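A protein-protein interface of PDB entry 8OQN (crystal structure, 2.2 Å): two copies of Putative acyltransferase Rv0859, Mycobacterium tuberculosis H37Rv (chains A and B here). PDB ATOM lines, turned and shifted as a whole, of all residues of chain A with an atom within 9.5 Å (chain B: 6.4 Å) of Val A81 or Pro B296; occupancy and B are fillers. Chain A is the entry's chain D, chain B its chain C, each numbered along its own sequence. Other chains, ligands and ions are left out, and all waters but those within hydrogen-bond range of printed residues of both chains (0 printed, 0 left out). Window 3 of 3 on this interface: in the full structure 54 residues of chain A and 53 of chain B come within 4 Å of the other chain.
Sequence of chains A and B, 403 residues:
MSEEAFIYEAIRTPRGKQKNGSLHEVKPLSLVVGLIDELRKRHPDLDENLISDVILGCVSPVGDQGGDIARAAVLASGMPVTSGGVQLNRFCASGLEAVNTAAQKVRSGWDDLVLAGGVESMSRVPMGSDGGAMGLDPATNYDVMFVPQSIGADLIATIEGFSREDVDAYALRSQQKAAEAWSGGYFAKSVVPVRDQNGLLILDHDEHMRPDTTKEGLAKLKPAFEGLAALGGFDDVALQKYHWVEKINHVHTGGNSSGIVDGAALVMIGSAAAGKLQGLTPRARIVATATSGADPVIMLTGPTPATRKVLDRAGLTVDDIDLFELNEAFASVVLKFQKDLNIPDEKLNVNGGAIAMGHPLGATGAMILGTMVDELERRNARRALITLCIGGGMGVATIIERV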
ATOM      1  N   ARG A  40     -32.141  25.496 -20.658  1.00  0.00           N
ATOM      2  CA  ARG A  40     -33.337  25.694 -19.846  1.00  0.00           C
ATOM      3  C   ARG A  40     -34.140  26.896 -20.325  1.00  0.00           C
ATOM      4  O   ARG A  40     -35.377  26.860 -20.324  1.00  0.00           O
ATOM      5  CB  ARG A  40     -32.953  25.861 -18.377  1.00  0.00           C
ATOM      6  CG  ARG A  40     -32.660  24.558 -17.664  1.00  0.00           C
ATOM      7  CD  ARG A  40     -31.919  24.802 -16.363  1.00  0.00           C
ATOM      8  NE  ARG A  40     -31.767  23.575 -15.590  1.00  0.00           N
ATOM      9  CZ  ARG A  40     -30.856  23.395 -14.645  1.00  0.00           C
ATOM     10  NH1 ARG A  40     -29.968  24.332 -14.351  1.00  0.00           N
ATOM     11  NH2 ARG A  40     -30.828  22.242 -13.981  1.00  0.00           N
ATOM     12  N   GLU A  48     -36.700  17.415 -16.999  1.00  0.00           N
ATOM     13  CA  GLU A  48     -35.306  16.992 -16.990  1.00  0.00           C
ATOM     14  C   GLU A  48     -35.114  15.578 -16.458  1.00  0.00           C
ATOM     15  O   GLU A  48     -34.024  15.020 -16.622  1.00  0.00           O
ATOM     16  CB  GLU A  48     -34.473  17.980 -16.173  1.00  0.00           C
ATOM     17  CG  GLU A  48     -34.493  19.396 -16.731  1.00  0.00           C
ATOM     18  CD  GLU A  48     -33.718  20.381 -15.876  1.00  0.00           C
ATOM     19  OE1 GLU A  48     -32.830  19.946 -15.114  1.00  0.00           O
ATOM     20  OE2 GLU A  48     -34.003  21.595 -15.967  1.00  0.00           O
ATOM     21  N   ASN A  49     -36.137  14.984 -15.835  1.00  0.00           N
ATOM     22  CA  ASN A  49     -36.024  13.601 -15.390  1.00  0.00           C
ATOM     23  C   ASN A  49     -35.932  12.628 -16.557  1.00  0.00           C
ATOM     24  O   ASN A  49     -35.459  11.502 -16.373  1.00  0.00           O
ATOM     25  CB  ASN A  49     -37.210  13.229 -14.497  1.00  0.00           C
ATOM     26  CG  ASN A  49     -37.310  14.106 -13.266  1.00  0.00           C
ATOM     27  OD1 ASN A  49     -36.462  14.045 -12.378  1.00  0.00           O
ATOM     28  ND2 ASN A  49     -38.357  14.921 -13.202  1.00  0.00           N
ATOM     29  N   ILE A  51     -33.952  13.016 -19.022  1.00  0.00           N
ATOM     30  CA  ILE A  51     -32.554  12.993 -19.437  1.00  0.00           C
ATOM     31  C   ILE A  51     -31.830  11.926 -18.626  1.00  0.00           C
ATOM     32  O   ILE A  51     -31.726  12.028 -17.398  1.00  0.00           O
ATOM     33  CB  ILE A  51     -31.898  14.367 -19.253  1.00  0.00           C
ATOM     34  CG1 ILE A  51     -32.588  15.403 -20.140  1.00  0.00           C
ATOM     35  CG2 ILE A  51     -30.413  14.294 -19.566  1.00  0.00           C
ATOM     36  CD1 ILE A  51     -32.063  16.805 -19.947  1.00  0.00           C
ATOM     37  N   SER A  52     -31.325  10.901 -19.311  1.00  0.00           N
ATOM     38  CA  SER A  52     -30.741   9.747 -18.644  1.00  0.00           C
ATOM     39  C   SER A  52     -29.220   9.784 -18.573  1.00  0.00           C
ATOM     40  O   SER A  52     -28.638   8.988 -17.829  1.00  0.00           O
ATOM     41  CB  SER A  52     -31.183   8.452 -19.341  1.00  0.00           C
ATOM     42  OG  SER A  52     -30.759   8.421 -20.693  1.00  0.00           O
ATOM     43  N   ASP A  53     -28.560  10.675 -19.311  1.00  0.00           N
ATOM     44  CA  ASP A  53     -27.105  10.713 -19.259  1.00  0.00           C
ATOM     45  C   ASP A  53     -26.594  12.045 -19.790  1.00  0.00           C
ATOM     46  O   ASP A  53     -27.258  12.712 -20.589  1.00  0.00           O
ATOM     47  CB  ASP A  53     -26.485   9.560 -20.055  1.00  0.00           C
ATOM     48  CG  ASP A  53     -25.274   8.962 -19.363  1.00  0.00           C
ATOM     49  OD1 ASP A  53     -24.705   9.633 -18.474  1.00  0.00           O
ATOM     50  OD2 ASP A  53     -24.900   7.819 -19.708  1.00  0.00           O
ATOM     51  N   VAL A  54     -25.401  12.416 -19.329  1.00  0.00           N
ATOM     52  CA  VAL A  54     -24.664  13.573 -19.823  1.00  0.00           C
ATOM     53  C   VAL A  54     -23.250  13.109 -20.144  1.00  0.00           C
ATOM     54  O   VAL A  54     -22.507  12.706 -19.241  1.00  0.00           O
ATOM     55  CB  VAL A  54     -24.639  14.727 -18.807  1.00  0.00           C
ATOM     56  CG1 VAL A  54     -23.699  15.823 -19.277  1.00  0.00           C
ATOM     57  CG2 VAL A  54     -26.042  15.278 -18.599  1.00  0.00           C
ATOM     58  N   ARG A  71     -20.471  14.617 -14.317  1.00  0.00           N
ATOM     59  CA  ARG A  71     -21.285  14.483 -13.115  1.00  0.00           C
ATOM     60  C   ARG A  71     -21.286  15.776 -12.312  1.00  0.00           C
ATOM     61  O   ARG A  71     -22.319  16.167 -11.757  1.00  0.00           O
ATOM     62  CB  ARG A  71     -20.785  13.316 -12.261  1.00  0.00           C
ATOM     63  CG  ARG A  71     -21.631  13.051 -11.022  1.00  0.00           C
ATOM     64  CD  ARG A  71     -23.088  12.854 -11.403  1.00  0.00           C
ATOM     65  NE  ARG A  71     -23.921  12.477 -10.268  1.00  0.00           N
ATOM     66  CZ  ARG A  71     -25.218  12.213 -10.354  1.00  0.00           C
ATOM     67  NH1 ARG A  71     -25.862  12.276 -11.509  1.00  0.00           N
ATOM     68  NH2 ARG A  71     -25.885  11.871  -9.256  1.00  0.00           N
ATOM     69  N   ALA A  72     -20.134  16.450 -12.239  1.00  0.00           N
ATOM     70  CA  ALA A  72     -20.072  17.751 -11.581  1.00  0.00           C
ATOM     71  C   ALA A  72     -21.043  18.734 -12.222  1.00  0.00           C
ATOM     72  O   ALA A  72     -21.711  19.506 -11.525  1.00  0.00           O
ATOM     73  CB  ALA A  72     -18.646  18.297 -11.634  1.00  0.00           C
ATOM     74  N   VAL A  74     -23.845  17.992 -13.866  1.00  0.00           N
ATOM     75  CA  VAL A  74     -25.207  17.598 -13.511  1.00  0.00           C
ATOM     76  C   VAL A  74     -25.571  18.144 -12.136  1.00  0.00           C
ATOM     77  O   VAL A  74     -26.644  18.729 -11.941  1.00  0.00           O
ATOM     78  CB  VAL A  74     -25.357  16.067 -13.564  1.00  0.00           C
ATOM     79  CG1 VAL A  74     -26.684  15.638 -12.954  1.00  0.00           C
ATOM     80  CG2 VAL A  74     -25.245  15.573 -14.994  1.00  0.00           C
ATOM     81  N   LEU A  75     -24.673  17.971 -11.164  1.00  0.00           N
ATOM     82  CA  LEU A  75     -24.975  18.366  -9.793  1.00  0.00           C
ATOM     83  C   LEU A  75     -24.925  19.880  -9.619  1.00  0.00           C
ATOM     84  O   LEU A  75     -25.803  20.461  -8.973  1.00  0.00           O
ATOM     85  CB  LEU A  75     -24.007  17.677  -8.830  1.00  0.00           C
ATOM     86  CG  LEU A  75     -24.040  16.147  -8.861  1.00  0.00           C
ATOM     87  CD1 LEU A  75     -23.038  15.565  -7.876  1.00  0.00           C
ATOM     88  CD2 LEU A  75     -25.446  15.633  -8.580  1.00  0.00           C
ATOM     89  N   ALA A  76     -23.911  20.536 -10.192  1.00  0.00           N
ATOM     90  CA  ALA A  76     -23.767  21.979 -10.013  1.00  0.00           C
ATOM     91  C   ALA A  76     -24.916  22.741 -10.660  1.00  0.00           C
ATOM     92  O   ALA A  76     -25.362  23.766 -10.130  1.00  0.00           O
ATOM     93  CB  ALA A  76     -22.428  22.449 -10.579  1.00  0.00           C
ATOM     94  N   SER A  77     -25.404  22.265 -11.804  1.00  0.00           N
ATOM     95  CA  SER A  77     -26.499  22.925 -12.502  1.00  0.00           C
ATOM     96  C   SER A  77     -27.862  22.603 -11.906  1.00  0.00           C
ATOM     97  O   SER A  77     -28.867  23.144 -12.377  1.00  0.00           O
ATOM     98  CB  SER A  77     -26.487  22.545 -13.986  1.00  0.00           C
ATOM     99  OG  SER A  77     -26.795  21.174 -14.172  1.00  0.00           O
ATOM    100  N   GLY A  78     -27.926  21.743 -10.893  1.00  0.00           N
ATOM    101  CA  GLY A  78     -29.207  21.400 -10.315  1.00  0.00           C
ATOM    102  C   GLY A  78     -30.057  20.488 -11.166  1.00  0.00           C
ATOM    103  O   GLY A  78     -31.278  20.459 -10.996  1.00  0.00           O
ATOM    104  N   MET A  79     -29.448  19.755 -12.096  1.00  0.00           N
ATOM    105  CA  MET A  79     -30.168  18.738 -12.839  1.00  0.00           C
ATOM    106  C   MET A  79     -30.519  17.576 -11.910  1.00  0.00           C
ATOM    107  O   MET A  79     -29.917  17.423 -10.844  1.00  0.00           O
ATOM    108  CB  MET A  79     -29.334  18.247 -14.021  1.00  0.00           C
ATOM    109  CG  MET A  79     -29.308  19.193 -15.210  1.00  0.00           C
ATOM    110  SD  MET A  79     -28.352  18.540 -16.592  1.00  0.00           S
ATOM    111  CE  MET A  79     -29.307  17.084 -17.013  1.00  0.00           C
ATOM    112  N   PRO A  80     -31.508  16.761 -12.278  1.00  0.00           N
ATOM    113  CA  PRO A  80     -31.871  15.620 -11.429  1.00  0.00           C
ATOM    114  C   PRO A  80     -30.692  14.683 -11.224  1.00  0.00           C
ATOM    115  O   PRO A  80     -29.861  14.493 -12.114  1.00  0.00           O
ATOM    116  CB  PRO A  80     -33.002  14.941 -12.208  1.00  0.00           C
ATOM    117  CG  PRO A  80     -33.577  16.021 -13.051  1.00  0.00           C
ATOM    118  CD  PRO A  80     -32.425  16.905 -13.423  1.00  0.00           C
ATOM    119  N   VAL A  81     -30.622  14.098 -10.026  1.00  0.00           N
ATOM    120  CA  VAL A  81     -29.528  13.196  -9.691  1.00  0.00           C
ATOM    121  C   VAL A  81     -29.576  11.896 -10.478  1.00  0.00           C
ATOM    122  O   VAL A  81     -28.604  11.132 -10.451  1.00  0.00           O
ATOM    123  CB  VAL A  81     -29.531  12.897  -8.180  1.00  0.00           C
ATOM    124  CG1 VAL A  81     -29.353  14.182  -7.388  1.00  0.00           C
ATOM    125  CG2 VAL A  81     -30.822  12.199  -7.785  1.00  0.00           C
ATOM    126  N   THR A  82     -30.675  11.627 -11.180  1.00  0.00           N
ATOM    127  CA  THR A  82     -30.785  10.445 -12.026  1.00  0.00           C
ATOM    128  C   THR A  82     -30.192  10.647 -13.413  1.00  0.00           C
ATOM    129  O   THR A  82     -30.277   9.733 -14.241  1.00  0.00           O
ATOM    130  CB  THR A  82     -32.253  10.027 -12.166  1.00  0.00           C
ATOM    131  OG1 THR A  82     -33.028  11.146 -12.615  1.00  0.00           O
ATOM    132  CG2 THR A  82     -32.802   9.530 -10.839  1.00  0.00           C
ATOM    133  N   SER A  83     -29.598  11.806 -13.689  1.00  0.00           N
ATOM    134  CA  SER A  83     -29.164  12.160 -15.033  1.00  0.00           C
ATOM    135  C   SER A  83     -27.743  11.706 -15.345  1.00  0.00           C
ATOM    136  O   SER A  83     -27.210  12.079 -16.393  1.00  0.00           O
ATOM    137  CB  SER A  83     -29.284  13.671 -15.247  1.00  0.00           C
ATOM    138  OG  SER A  83     -30.642  14.072 -15.251  1.00  0.00           O
ATOM    139  N   GLY A  84     -27.122  10.924 -14.464  1.00  0.00           N
ATOM    140  CA  GLY A  84     -25.824  10.346 -14.781  1.00  0.00           C
ATOM    141  C   GLY A  84     -24.737  11.394 -14.946  1.00  0.00           C
ATOM    142  O   GLY A  84     -24.618  12.335 -14.154  1.00  0.00           O
ATOM    143  N   GLY A  85     -23.931  11.230 -15.994  1.00  0.00           N
ATOM    144  CA  GLY A  85     -22.775  12.079 -16.222  1.00  0.00           C
ATOM    145  C   GLY A  85     -21.498  11.272 -16.335  1.00  0.00           C
ATOM    146  O   GLY A  85     -21.041  10.686 -15.350  1.00  0.00           O
ATOM    147  N   MET B 134     -15.920  18.869  -7.826  1.00  0.00           N
ATOM    148  CA  MET B 134     -16.828  18.524  -6.737  1.00  0.00           C
ATOM    149  C   MET B 134     -16.141  18.500  -5.379  1.00  0.00           C
ATOM    150  O   MET B 134     -16.814  18.645  -4.350  1.00  0.00           O
ATOM    151  CB  MET B 134     -17.468  17.159  -7.003  1.00  0.00           C
ATOM    152  CG  MET B 134     -18.653  17.177  -7.954  1.00  0.00           C
ATOM    153  SD  MET B 134     -19.118  15.512  -8.473  1.00  0.00           S
ATOM    154  CE  MET B 134     -19.090  14.648  -6.904  1.00  0.00           C
ATOM    155  N   VAL B 144     -23.157  21.554  -3.236  1.00  0.00           N
ATOM    156  CA  VAL B 144     -23.656  20.186  -3.371  1.00  0.00           C
ATOM    157  C   VAL B 144     -23.490  19.369  -2.101  1.00  0.00           C
ATOM    158  O   VAL B 144     -23.952  18.221  -2.055  1.00  0.00           O
ATOM    159  CB  VAL B 144     -22.959  19.444  -4.525  1.00  0.00           C
ATOM    160  CG1 VAL B 144     -23.040  20.263  -5.799  1.00  0.00           C
ATOM    161  CG2 VAL B 144     -21.517  19.138  -4.161  1.00  0.00           C
ATOM    162  N   MET B 145     -22.837  19.925  -1.080  1.00  0.00           N
ATOM    163  CA  MET B 145     -22.652  19.271   0.215  1.00  0.00           C
ATOM    164  C   MET B 145     -21.911  17.941   0.053  1.00  0.00           C
ATOM    165  O   MET B 145     -22.431  16.860   0.337  1.00  0.00           O
ATOM    166  CB  MET B 145     -23.998  19.087   0.927  1.00  0.00           C
ATOM    167  CG  MET B 145     -24.830  20.364   0.986  1.00  0.00           C
ATOM    168  SD  MET B 145     -26.450  20.144   1.751  1.00  0.00           S
ATOM    169  CE  MET B 145     -26.011  20.050   3.486  1.00  0.00           C
ATOM    170  N   PHE B 146     -20.669  18.049  -0.417  1.00  0.00           N
ATOM    171  CA  PHE B 146     -19.849  16.872  -0.673  1.00  0.00           C
ATOM    172  C   PHE B 146     -19.535  16.133   0.622  1.00  0.00           C
ATOM    173  O   PHE B 146     -19.178  16.742   1.635  1.00  0.00           O
ATOM    174  CB  PHE B 146     -18.555  17.279  -1.377  1.00  0.00           C
ATOM    175  CG  PHE B 146     -17.511  16.198  -1.402  1.00  0.00           C
ATOM    176  CD1 PHE B 146     -17.642  15.109  -2.246  1.00  0.00           C
ATOM    177  CD2 PHE B 146     -16.394  16.274  -0.584  1.00  0.00           C
ATOM    178  CE1 PHE B 146     -16.683  14.113  -2.270  1.00  0.00           C
ATOM    179  CE2 PHE B 146     -15.431  15.282  -0.606  1.00  0.00           C
ATOM    180  CZ  PHE B 146     -15.576  14.200  -1.449  1.00  0.00           C
ATOM    181  N   VAL B 147     -19.668  14.810   0.580  1.00  0.00           N
ATOM    182  CA  VAL B 147     -19.391  13.940   1.721  1.00  0.00           C
ATOM    183  C   VAL B 147     -18.695  12.682   1.210  1.00  0.00           C
ATOM    184  O   VAL B 147     -19.122  12.112   0.196  1.00  0.00           O
ATOM    185  CB  VAL B 147     -20.680  13.596   2.487  1.00  0.00           C
ATOM    186  CG1 VAL B 147     -20.457  12.409   3.408  1.00  0.00           C
ATOM    187  CG2 VAL B 147     -21.162  14.797   3.285  1.00  0.00           C
ATOM    188  N   LYS B 241     -28.190  17.779   5.826  1.00  0.00           N
ATOM    189  CA  LYS B 241     -29.179  17.325   4.858  1.00  0.00           C
ATOM    190  C   LYS B 241     -30.092  16.253   5.443  1.00  0.00           C
ATOM    191  O   LYS B 241     -31.313  16.312   5.270  1.00  0.00           O
ATOM    192  CB  LYS B 241     -28.499  16.798   3.592  1.00  0.00           C
ATOM    193  CG  LYS B 241     -29.508  16.328   2.560  1.00  0.00           C
ATOM    194  CD  LYS B 241     -28.882  16.010   1.226  1.00  0.00           C
ATOM    195  CE  LYS B 241     -29.958  15.818   0.168  1.00  0.00           C
ATOM    196  NZ  LYS B 241     -30.018  16.961  -0.786  1.00  0.00           N
ATOM    197  N   TYR B 242     -29.523  15.268   6.134  1.00  0.00           N
ATOM    198  CA  TYR B 242     -30.317  14.217   6.770  1.00  0.00           C
ATOM    199  C   TYR B 242     -30.616  14.634   8.210  1.00  0.00           C
ATOM    200  O   TYR B 242     -30.142  14.052   9.189  1.00  0.00           O
ATOM    201  CB  TYR B 242     -29.597  12.879   6.677  1.00  0.00           C
ATOM    202  CG  TYR B 242     -29.587  12.343   5.261  1.00  0.00           C
ATOM    203  CD1 TYR B 242     -28.626  12.756   4.345  1.00  0.00           C
ATOM    204  CD2 TYR B 242     -30.559  11.449   4.831  1.00  0.00           C
ATOM    205  CE1 TYR B 242     -28.624  12.283   3.046  1.00  0.00           C
ATOM    206  CE2 TYR B 242     -30.565  10.970   3.533  1.00  0.00           C
ATOM    207  CZ  TYR B 242     -29.597  11.389   2.646  1.00  0.00           C
ATOM    208  OH  TYR B 242     -29.607  10.911   1.356  1.00  0.00           O
ATOM    209  N   SER B 292     -29.291   5.165 -13.645  1.00  0.00           N
ATOM    210  CA  SER B 292     -30.137   6.032 -12.835  1.00  0.00           C
ATOM    211  C   SER B 292     -29.283   6.578 -11.694  1.00  0.00           C
ATOM    212  O   SER B 292     -28.050   6.578 -11.771  1.00  0.00           O
ATOM    213  CB  SER B 292     -31.382   5.266 -12.358  1.00  0.00           C
ATOM    214  OG  SER B 292     -32.323   6.143 -11.767  1.00  0.00           O
ATOM    215  N   GLY B 293     -29.933   7.046 -10.633  1.00  0.00           N
ATOM    216  CA  GLY B 293     -29.185   7.591  -9.517  1.00  0.00           C
ATOM    217  C   GLY B 293     -30.092   7.935  -8.357  1.00  0.00           C
ATOM    218  O   GLY B 293     -31.315   7.784  -8.423  1.00  0.00           O
ATOM    219  N   ALA B 294     -29.463   8.399  -7.283  1.00  0.00           N
ATOM    220  CA  ALA B 294     -30.163   8.815  -6.074  1.00  0.00           C
ATOM    221  C   ALA B 294     -29.370   9.954  -5.438  1.00  0.00           C
ATOM    222  O   ALA B 294     -28.539  10.591  -6.095  1.00  0.00           O
ATOM    223  CB  ALA B 294     -30.365   7.619  -5.128  1.00  0.00           C
ATOM    224  N   ASP B 295     -29.617  10.204  -4.155  1.00  0.00           N
ATOM    225  CA  ASP B 295     -29.039  11.363  -3.487  1.00  0.00           C
ATOM    226  C   ASP B 295     -27.515  11.266  -3.454  1.00  0.00           C
ATOM    227  O   ASP B 295     -26.972  10.233  -3.038  1.00  0.00           O
ATOM    228  CB  ASP B 295     -29.592  11.485  -2.068  1.00  0.00           C
ATOM    229  CG  ASP B 295     -28.844  12.509  -1.242  1.00  0.00           C
ATOM    230  OD1 ASP B 295     -28.750  13.672  -1.684  1.00  0.00           O
ATOM    231  OD2 ASP B 295     -28.346  12.147  -0.154  1.00  0.00           O
ATOM    232  N   PRO B 296     -26.793  12.312  -3.875  1.00  0.00           N
ATOM    233  CA  PRO B 296     -25.325  12.243  -3.891  1.00  0.00           C
ATOM    234  C   PRO B 296     -24.667  12.503  -2.546  1.00  0.00           C
ATOM    235  O   PRO B 296     -23.450  12.301  -2.428  1.00  0.00           O
ATOM    236  CB  PRO B 296     -24.944  13.330  -4.901  1.00  0.00           C
ATOM    237  CG  PRO B 296     -26.034  14.335  -4.773  1.00  0.00           C
ATOM    238  CD  PRO B 296     -27.295  13.557  -4.482  1.00  0.00           C
ATOM    239  N   VAL B 297     -25.412  12.956  -1.536  1.00  0.00           N
ATOM    240  CA  VAL B 297     -24.821  13.110  -0.211  1.00  0.00           C
ATOM    241  C   VAL B 297     -24.714  11.758   0.482  1.00  0.00           C
ATOM    242  O   VAL B 297     -23.686  11.440   1.090  1.00  0.00           O
ATOM    243  CB  VAL B 297     -25.627  14.122   0.622  1.00  0.00           C
ATOM    244  CG1 VAL B 297     -25.069  14.208   2.034  1.00  0.00           C
ATOM    245  CG2 VAL B 297     -25.597  15.487  -0.046  1.00  0.00           C
ATOM    246  N   ILE B 298     -25.767  10.939   0.397  1.00  0.00           N
ATOM    247  CA  ILE B 298     -25.669   9.564   0.875  1.00  0.00           C
ATOM    248  C   ILE B 298     -24.872   8.724  -0.120  1.00  0.00           C
ATOM    249  O   ILE B 298     -24.218   7.746   0.262  1.00  0.00           O
ATOM    250  CB  ILE B 298     -27.077   8.998   1.145  1.00  0.00           C
ATOM    251  CG1 ILE B 298     -27.023   7.847   2.151  1.00  0.00           C
ATOM    252  CG2 ILE B 298     -27.760   8.559  -0.143  1.00  0.00           C
ATOM    253  CD1 ILE B 298     -28.391   7.422   2.647  1.00  0.00           C
ATOM    254  N   MET B 299     -24.934   9.080  -1.407  1.00  0.00           N
ATOM    255  CA  MET B 299     -23.939   8.732  -2.420  1.00  0.00           C
ATOM    256  C   MET B 299     -23.864   7.251  -2.792  1.00  0.00           C
ATOM    257  O   MET B 299     -23.212   6.906  -3.782  1.00  0.00           O
ATOM    258  CB  MET B 299     -22.558   9.212  -1.963  1.00  0.00           C
ATOM    259  CG  MET B 299     -21.598   9.531  -3.098  1.00  0.00           C
ATOM    260  SD  MET B 299     -19.952   9.996  -2.526  1.00  0.00           S
ATOM    261  CE  MET B 299     -19.606  11.377  -3.613  1.00  0.00           C
ATOM    262  N   LEU B 300     -24.503   6.361  -2.031  1.00  0.00           N
ATOM    263  CA  LEU B 300     -24.378   4.931  -2.297  1.00  0.00           C
ATOM    264  C   LEU B 300     -25.717   4.242  -2.545  1.00  0.00           C
ATOM    265  O   LEU B 300     -25.762   3.007  -2.591  1.00  0.00           O
ATOM    266  CB  LEU B 300     -23.650   4.229  -1.148  1.00  0.00           C
ATOM    267  CG  LEU B 300     -22.135   4.420  -0.995  1.00  0.00           C
ATOM    268  CD1 LEU B 300     -21.433   4.461  -2.351  1.00  0.00           C
ATOM    269  CD2 LEU B 300     -21.802   5.649  -0.163  1.00  0.00           C
ATOM    270  N   THR B 301     -26.801   4.993  -2.726  1.00  0.00           N
ATOM    271  CA  THR B 301     -28.120   4.410  -2.901  1.00  0.00           C
ATOM    272  C   THR B 301     -28.558   4.343  -4.364  1.00  0.00           C
ATOM    273  O   THR B 301     -29.716   3.996  -4.638  1.00  0.00           O
ATOM    274  CB  THR B 301     -29.150   5.189  -2.086  1.00  0.00           C
ATOM    275  OG1 THR B 301     -29.055   6.585  -2.394  1.00  0.00           O
ATOM    276  CG2 THR B 301     -28.907   4.984  -0.599  1.00  0.00           C
ATOM    277  N   GLY B 391     -19.949   6.918  -7.014  1.00  0.00           N
ATOM    278  CA  GLY B 391     -19.787   8.246  -6.455  1.00  0.00           C
ATOM    279  C   GLY B 391     -20.666   9.256  -7.167  1.00  0.00           C
ATOM    280  O   GLY B 391     -20.993   9.112  -8.347  1.00  0.00           O
ATOM    281  N   GLY B 392     -21.055  10.295  -6.434  1.00  0.00           N
ATOM    282  CA  GLY B 392     -21.997  11.259  -6.962  1.00  0.00           C
ATOM    283  C   GLY B 392     -23.436  10.796  -6.971  1.00  0.00           C
ATOM    284  O   GLY B 392     -24.290  11.491  -7.533  1.00  0.00           O
ATOM    285  N   GLY B 393     -23.729   9.642  -6.376  1.00  0.00           N
ATOM    286  CA  GLY B 393     -25.093   9.166  -6.274  1.00  0.00           C
ATOM    287  C   GLY B 393     -25.649   8.500  -7.510  1.00  0.00           C
ATOM    288  O   GLY B 393     -26.871   8.429  -7.658  1.00  0.00           O
ATOM    289  N   MET B 394     -24.796   8.004  -8.401  1.00  0.00           N
ATOM    290  CA  MET B 394     -25.249   7.389  -9.639  1.00  0.00           C
ATOM    291  C   MET B 394     -25.460   5.886  -9.457  1.00  0.00           C
ATOM    292  O   MET B 394     -25.140   5.303  -8.419  1.00  0.00           O
ATOM    293  CB  MET B 394     -24.246   7.656 -10.763  1.00  0.00           C
ATOM    294  CG  MET B 394     -24.142   9.111 -11.183  1.00  0.00           C
ATOM    295  SD  MET B 394     -22.945   9.381 -12.506  1.00  0.00           S
ATOM    296  CE  MET B 394     -21.399   9.275 -11.608  1.00  0.00           C
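Printed residues of chain A that touch a printed residue of chain B: Arg A71, Ala A72, Leu A75, Val A81, Thr A82, Gly A84 and Gly A85. Hydrophobic or aromatic side chains of chain A within 4 Å of the printed part of chain B: Ala A72, Leu A75 and Val A81. Hydrophobic or aromatic side chains of chain B that line the printed part of chain A: Met B134, Pro B296 and Met B394. Among the printed residues, no Asp or Glu carboxylate lies within 4 Å of a Lys or Arg side-chain nitrogen of the other chain.
No position is printed for both chains.
Arg A71 touches Gly B393. Arg A71 touches Met B394 (CZ to CG, 3.4 Å). Ala A72 touches Met B134 (CB to CG, 3.8 Å). CD1 of Leu A75 touches SD of Met B134, at 3.97 Å. Val A81 touches Gly B293 (O to CA, 3.7 Å). Ala B294 touches Val A81. Pro B296 touches Val A81. CG2 of Thr A82 touches OG of Ser B292, at 3.5 Å. Thr A82 touches Gly B293.
The backbone carbonyl oxygen (O) of Gly B392 sits at hydrogen-bond distance from the guanidinium group (NE) of Arg A71, at 2.9 Å. The backbone carbonyl oxygen of Gly A84 lies close to the side-chain sulfur of Met B394, at 3.8 Å. The backbone carbonyl oxygen (O) of Gly A85 lies close to the side-chain sulfur (SD) of Met B394.
N of Ala B294 is in hydrogen-bond range of O of Gly B393, at 2.6 Å. OD1 of Asp A53 sits at hydrogen-bond distance from N of Gly A85, at 3.0 Å. NH2 of Arg A71 sits at hydrogen-bond distance from O of Val A81, at 3.1 Å. The guanidinium group (NH1) of Arg A71 is in hydrogen-bond range of the backbone carbonyl oxygen (O) of Gly A84 (2.9 Å).
Of the printed residues of chain B, Ala A72 touches Met B134 (3.8 Å). Of the printed residues of chain B, Leu A75 touches Met B134. Of chain B, only Gly B293 (3.7 Å), Ala B294 (3.3 Å) and Pro B296 (3.6 Å) come within 4 Å of Val A81. Printed residues of chain B within 4 Å of Gly A84: Met B394 (3.6 Å). Printed residues of chain B within 4 Å of Gly A85: Met B394 (3.7 Å). Gly B293 touches just these residues of chain A: Val A81 (3.7 Å) and Thr A82 (3.3 Å). Printed residues of chain A within 4 Å of Ala B294: Val A81 (3.3 Å). No residue of chain A comes within 4 Å of Asp B295. Of the printed residues of chain A, Pro B296 touches Val A81. No residue of chain A comes within 4 Å of Val B297. Gly B392 touches one residue of chain A. Of chain A, only Arg A71 (3.8 Å) comes within 4 Å of Gly B393. Of the printed residues of chain A, Met B394 touches Arg A71, Gly A84 and Gly A85. The nearest residue of chain B that does not touch Val A81 is Gly B393 (4.3 Å). The nearest residue of chain A that does not touch Pro B296 is Leu A75 (4.1 Å).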
